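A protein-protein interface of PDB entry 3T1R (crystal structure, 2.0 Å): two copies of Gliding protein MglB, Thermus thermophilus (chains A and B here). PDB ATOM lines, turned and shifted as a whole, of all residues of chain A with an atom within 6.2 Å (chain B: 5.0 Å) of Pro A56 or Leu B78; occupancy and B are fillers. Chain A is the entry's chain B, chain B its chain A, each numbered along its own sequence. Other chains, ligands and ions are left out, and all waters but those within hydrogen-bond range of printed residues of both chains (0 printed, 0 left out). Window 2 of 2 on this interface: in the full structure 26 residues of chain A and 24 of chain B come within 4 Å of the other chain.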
ATOM      1  N   TYR A  33      -5.214 -33.293 -12.911  1.00  0.00           N
ATOM      2  CA  TYR A  33      -4.041 -33.087 -13.821  1.00  0.00           C
ATOM      3  C   TYR A  33      -2.855 -32.662 -12.947  1.00  0.00           C
ATOM      4  O   TYR A  33      -3.048 -31.890 -11.992  1.00  0.00           O
ATOM      5  CB  TYR A  33      -4.294 -32.021 -14.891  1.00  0.00           C
ATOM      6  CG  TYR A  33      -5.687 -32.144 -15.496  1.00  0.00           C
ATOM      7  CD1 TYR A  33      -6.119 -33.356 -16.067  1.00  0.00           C
ATOM      8  CD2 TYR A  33      -6.619 -31.065 -15.378  1.00  0.00           C
ATOM      9  CE1 TYR A  33      -7.413 -33.468 -16.618  1.00  0.00           C
ATOM     10  CE2 TYR A  33      -7.965 -31.211 -15.864  1.00  0.00           C
ATOM     11  CZ  TYR A  33      -8.312 -32.422 -16.501  1.00  0.00           C
ATOM     12  OH  TYR A  33      -9.597 -32.597 -17.038  1.00  0.00           O
ATOM     13  N   LYS A  54     -10.807 -34.719 -20.722  1.00  0.00           N
ATOM     14  CA  LYS A  54      -9.753 -33.990 -21.407  1.00  0.00           C
ATOM     15  C   LYS A  54      -9.425 -32.669 -20.688  1.00  0.00           C
ATOM     16  O   LYS A  54     -10.335 -31.919 -20.365  1.00  0.00           O
ATOM     17  CB  LYS A  54     -10.216 -33.683 -22.828  1.00  0.00           C
ATOM     18  CG  LYS A  54      -9.192 -33.017 -23.675  1.00  0.00           C
ATOM     19  CD  LYS A  54      -9.777 -32.805 -25.094  1.00  0.00           C
ATOM     20  CE  LYS A  54      -8.908 -31.839 -25.890  1.00  0.00           C
ATOM     21  NZ  LYS A  54      -9.710 -31.083 -26.927  1.00  0.00           N
ATOM     22  N   PRO A  55      -8.139 -32.363 -20.469  1.00  0.00           N
ATOM     23  CA  PRO A  55      -7.930 -31.171 -19.666  1.00  0.00           C
ATOM     24  C   PRO A  55      -8.148 -29.924 -20.497  1.00  0.00           C
ATOM     25  O   PRO A  55      -8.229 -30.005 -21.722  1.00  0.00           O
ATOM     26  CB  PRO A  55      -6.423 -31.289 -19.284  1.00  0.00           C
ATOM     27  CG  PRO A  55      -5.792 -32.064 -20.484  1.00  0.00           C
ATOM     28  CD  PRO A  55      -6.884 -33.136 -20.593  1.00  0.00           C
ATOM     29  N   PRO A  56      -8.193 -28.755 -19.855  1.00  0.00           N
ATOM     30  CA  PRO A  56      -8.009 -27.571 -20.689  1.00  0.00           C
ATOM     31  C   PRO A  56      -6.587 -27.527 -21.332  1.00  0.00           C
ATOM     32  O   PRO A  56      -5.671 -28.265 -20.953  1.00  0.00           O
ATOM     33  CB  PRO A  56      -8.192 -26.437 -19.677  1.00  0.00           C
ATOM     34  CG  PRO A  56      -7.549 -26.980 -18.476  1.00  0.00           C
ATOM     35  CD  PRO A  56      -8.128 -28.394 -18.420  1.00  0.00           C
ATOM     36  N   PRO A  57      -6.394 -26.674 -22.355  1.00  0.00           N
ATOM     37  CA  PRO A  57      -5.061 -26.645 -22.993  1.00  0.00           C
ATOM     38  C   PRO A  57      -3.925 -26.488 -21.978  1.00  0.00           C
ATOM     39  O   PRO A  57      -3.861 -25.494 -21.242  1.00  0.00           O
ATOM     40  CB  PRO A  57      -5.111 -25.410 -23.914  1.00  0.00           C
ATOM     41  CG  PRO A  57      -6.572 -25.108 -24.093  1.00  0.00           C
ATOM     42  CD  PRO A  57      -7.384 -25.759 -22.969  1.00  0.00           C
ATOM     43  N   LEU A  58      -3.025 -27.458 -21.912  1.00  0.00           N
ATOM     44  CA  LEU A  58      -2.139 -27.487 -20.743  1.00  0.00           C
ATOM     45  C   LEU A  58      -1.031 -26.501 -20.965  1.00  0.00           C
ATOM     46  O   LEU A  58      -0.424 -26.046 -19.990  1.00  0.00           O
ATOM     47  CB  LEU A  58      -1.531 -28.878 -20.515  1.00  0.00           C
ATOM     48  CG  LEU A  58      -2.536 -29.912 -20.012  1.00  0.00           C
ATOM     49  CD1 LEU A  58      -1.849 -31.347 -19.911  1.00  0.00           C
ATOM     50  CD2 LEU A  58      -3.110 -29.474 -18.669  1.00  0.00           C
ATOM     51  N   ASP A  59      -0.737 -26.163 -22.238  1.00  0.00           N
ATOM     52  CA  ASP A  59       0.352 -25.157 -22.461  1.00  0.00           C
ATOM     53  C   ASP A  59      -0.129 -23.800 -21.977  1.00  0.00           C
ATOM     54  O   ASP A  59       0.632 -23.058 -21.341  1.00  0.00           O
ATOM     55  CB  ASP A  59       0.885 -25.093 -23.957  1.00  0.00           C
ATOM     56  CG  ASP A  59      -0.232 -25.000 -24.978  1.00  0.00           C
ATOM     57  OD1 ASP A  59      -1.432 -25.305 -24.655  1.00  0.00           O
ATOM     58  OD2 ASP A  59       0.058 -24.547 -26.119  1.00  0.00           O
ATOM     59  N   THR A  60      -1.394 -23.493 -22.240  1.00  0.00           N
ATOM     60  CA  THR A  60      -1.982 -22.232 -21.734  1.00  0.00           C
ATOM     61  C   THR A  60      -2.082 -22.195 -20.206  1.00  0.00           C
ATOM     62  O   THR A  60      -1.835 -21.179 -19.559  1.00  0.00           O
ATOM     63  CB  THR A  60      -3.399 -22.057 -22.279  1.00  0.00           C
ATOM     64  OG1 THR A  60      -3.352 -22.306 -23.683  1.00  0.00           O
ATOM     65  CG2 THR A  60      -3.910 -20.623 -22.027  1.00  0.00           C
ATOM     66  N   LEU A  61      -2.425 -23.324 -19.622  1.00  0.00           N
ATOM     67  CA  LEU A  61      -2.479 -23.405 -18.146  1.00  0.00           C
ATOM     68  C   LEU A  61      -1.099 -23.134 -17.561  1.00  0.00           C
ATOM     69  O   LEU A  61      -1.009 -22.413 -16.617  1.00  0.00           O
ATOM     70  CB  LEU A  61      -2.964 -24.824 -17.732  1.00  0.00           C
ATOM     71  CG  LEU A  61      -2.839 -25.073 -16.212  1.00  0.00           C
ATOM     72  CD1 LEU A  61      -3.948 -24.335 -15.656  1.00  0.00           C
ATOM     73  CD2 LEU A  61      -2.940 -26.566 -15.806  1.00  0.00           C
ATOM     74  N   ALA A  62      -0.032 -23.744 -18.077  1.00  0.00           N
ATOM     75  CA  ALA A  62       1.340 -23.505 -17.580  1.00  0.00           C
ATOM     76  C   ALA A  62       1.790 -22.039 -17.765  1.00  0.00           C
ATOM     77  O   ALA A  62       2.510 -21.489 -16.907  1.00  0.00           O
ATOM     78  CB  ALA A  62       2.314 -24.398 -18.321  1.00  0.00           C
ATOM     79  N   LEU A  64      -0.189 -19.240 -17.961  1.00  0.00           N
ATOM     80  CA  LEU A  64      -0.914 -18.424 -17.032  1.00  0.00           C
ATOM     81  C   LEU A  64      -0.403 -18.627 -15.575  1.00  0.00           C
ATOM     82  O   LEU A  64      -0.344 -17.652 -14.790  1.00  0.00           O
ATOM     83  CB  LEU A  64      -2.422 -18.749 -17.155  1.00  0.00           C
ATOM     84  CG  LEU A  64      -3.106 -18.249 -18.428  1.00  0.00           C
ATOM     85  CD1 LEU A  64      -4.569 -18.691 -18.341  1.00  0.00           C
ATOM     86  CD2 LEU A  64      -2.989 -16.677 -18.625  1.00  0.00           C
ATOM     87  N   VAL A 110      -4.213 -29.680 -10.547  1.00  0.00           N
ATOM     88  CA  VAL A 110      -5.555 -29.120 -10.832  1.00  0.00           C
ATOM     89  C   VAL A 110      -6.513 -30.126 -10.270  1.00  0.00           C
ATOM     90  O   VAL A 110      -6.385 -31.321 -10.591  1.00  0.00           O
ATOM     91  CB  VAL A 110      -5.817 -29.013 -12.378  1.00  0.00           C
ATOM     92  CG1 VAL A 110      -7.342 -28.537 -12.703  1.00  0.00           C
ATOM     93  CG2 VAL A 110      -4.723 -28.141 -13.065  1.00  0.00           C
ATOM     94  N   ALA B  74      -8.182 -14.924 -15.560  1.00  0.00           N
ATOM     95  CA  ALA B  74      -8.001 -15.690 -16.815  1.00  0.00           C
ATOM     96  C   ALA B  74      -7.739 -17.190 -16.531  1.00  0.00           C
ATOM     97  O   ALA B  74      -8.239 -18.066 -17.207  1.00  0.00           O
ATOM     98  CB  ALA B  74      -6.873 -15.088 -17.673  1.00  0.00           C
ATOM     99  N   LEU B  75      -6.938 -17.455 -15.523  1.00  0.00           N
ATOM    100  CA  LEU B  75      -6.654 -18.787 -15.131  1.00  0.00           C
ATOM    101  C   LEU B  75      -7.916 -19.471 -14.618  1.00  0.00           C
ATOM    102  O   LEU B  75      -8.136 -20.664 -14.921  1.00  0.00           O
ATOM    103  CB  LEU B  75      -5.640 -18.758 -14.001  1.00  0.00           C
ATOM    104  CG  LEU B  75      -4.408 -19.625 -13.985  1.00  0.00           C
ATOM    105  CD1 LEU B  75      -3.808 -19.531 -12.597  1.00  0.00           C
ATOM    106  CD2 LEU B  75      -4.700 -21.057 -14.448  1.00  0.00           C
ATOM    107  N   ALA B  76      -8.697 -18.786 -13.772  1.00  0.00           N
ATOM    108  CA  ALA B  76      -9.984 -19.360 -13.320  1.00  0.00           C
ATOM    109  C   ALA B  76     -10.919 -19.748 -14.477  1.00  0.00           C
ATOM    110  O   ALA B  76     -11.602 -20.810 -14.410  1.00  0.00           O
ATOM    111  CB  ALA B  76     -10.754 -18.400 -12.358  1.00  0.00           C
ATOM    112  N   LYS B  77     -10.966 -18.870 -15.491  1.00  0.00           N
ATOM    113  CA  LYS B  77     -11.860 -19.091 -16.644  1.00  0.00           C
ATOM    114  C   LYS B  77     -11.425 -20.279 -17.471  1.00  0.00           C
ATOM    115  O   LYS B  77     -12.267 -21.070 -17.947  1.00  0.00           O
ATOM    116  CB  LYS B  77     -11.966 -17.838 -17.505  1.00  0.00           C
ATOM    117  CG  LYS B  77     -12.821 -16.745 -16.883  1.00  0.00           C
ATOM    118  CD  LYS B  77     -12.718 -15.508 -17.852  1.00  0.00           C
ATOM    119  CE  LYS B  77     -13.855 -14.525 -17.587  1.00  0.00           C
ATOM    120  NZ  LYS B  77     -13.959 -14.159 -16.128  1.00  0.00           N
ATOM    121  N   LEU B  78     -10.122 -20.480 -17.549  1.00  0.00           N
ATOM    122  CA  LEU B  78      -9.580 -21.664 -18.189  1.00  0.00           C
ATOM    123  C   LEU B  78     -10.023 -22.933 -17.455  1.00  0.00           C
ATOM    124  O   LEU B  78     -10.239 -23.959 -18.121  1.00  0.00           O
ATOM    125  CB  LEU B  78      -8.053 -21.580 -18.261  1.00  0.00           C
ATOM    126  CG  LEU B  78      -7.263 -22.519 -19.114  1.00  0.00           C
ATOM    127  CD1 LEU B  78      -7.583 -22.171 -20.581  1.00  0.00           C
ATOM    128  CD2 LEU B  78      -5.703 -22.438 -18.811  1.00  0.00           C
ATOM    129  N   LEU B  79     -10.166 -22.881 -16.124  1.00  0.00           N
ATOM    130  CA  LEU B  79     -10.743 -23.999 -15.362  1.00  0.00           C
ATOM    131  C   LEU B  79     -12.284 -24.005 -15.339  1.00  0.00           C
ATOM    132  O   LEU B  79     -12.892 -24.824 -14.683  1.00  0.00           O
ATOM    133  CB  LEU B  79     -10.145 -24.017 -13.940  1.00  0.00           C
ATOM    134  CG  LEU B  79      -8.610 -23.895 -14.041  1.00  0.00           C
ATOM    135  CD1 LEU B  79      -7.938 -23.763 -12.603  1.00  0.00           C
ATOM    136  CD2 LEU B  79      -8.022 -25.124 -14.711  1.00  0.00           C
ATOM    137  N   GLY B  80     -12.933 -23.092 -16.053  1.00  0.00           N
ATOM    138  CA  GLY B  80     -14.360 -23.146 -16.136  1.00  0.00           C
ATOM    139  C   GLY B  80     -15.075 -22.279 -15.137  1.00  0.00           C
ATOM    140  O   GLY B  80     -16.258 -22.490 -14.922  1.00  0.00           O
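CB of Pro A56 touches O of Leu B78, at 3.6 Å. Leu B78 touches Thr A60. Leu A61 touches Leu B75. CD2 of Leu B78 touches CA of Leu A61 (3.4 Å). Leu A64 touches Ala B74 (CD1 to O, 3.9 Å). Leu A64 touches Leu B75 (CD1 to CA, 3.8 Å). Leu A64 touches Leu B78 (CD1 to CD2, 3.9 Å).
No position is printed for both chains.
Hydrophobic or aromatic side chains of chain B that line the printed part of chain A: Leu B75 and Leu B78. Along chain B the printed residues that touch a printed residue of chain A span positions 74 to 78. Among the printed residues, 7 pairs touch across the chains. Among the printed residues, no Asp or Glu carboxylate lies within 4 Å of a Lys or Arg side-chain nitrogen of the other chain.
Of chain B, only Leu B78 (3.6 Å) comes within 4 Å of Pro A56. Of the printed residues of chain B, Thr A60 touches Leu B78 (3.9 Å). Printed residues of chain B within 4 Å of Leu A61: Leu B75 (3.6 Å) and Leu B78 (3.4 Å). Of the printed residues of chain B, Leu A64 touches Ala B74 (3.9 Å), Leu B75 (3.8 Å) and Leu B78 (3.9 Å). Of the printed residues of chain A, Ala B74 touches Leu A64. Of the printed residues of chain A, Leu B75 touches Leu A61 (3.6 Å) and Leu A64 (3.8 Å). Leu B78 touches just these residues of chain A: Pro A56, Thr A60, Leu A61 and Leu A64. The nearest residue of chain B that does not touch Pro A56 is Leu B79 (4.2 Å). The nearest residue of chain A that does not touch Leu B78 is Pro A57 (4.3 Å). The nearest printed residue of chain B that does not touch Leu A61 is Leu B79 (4.3 Å).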
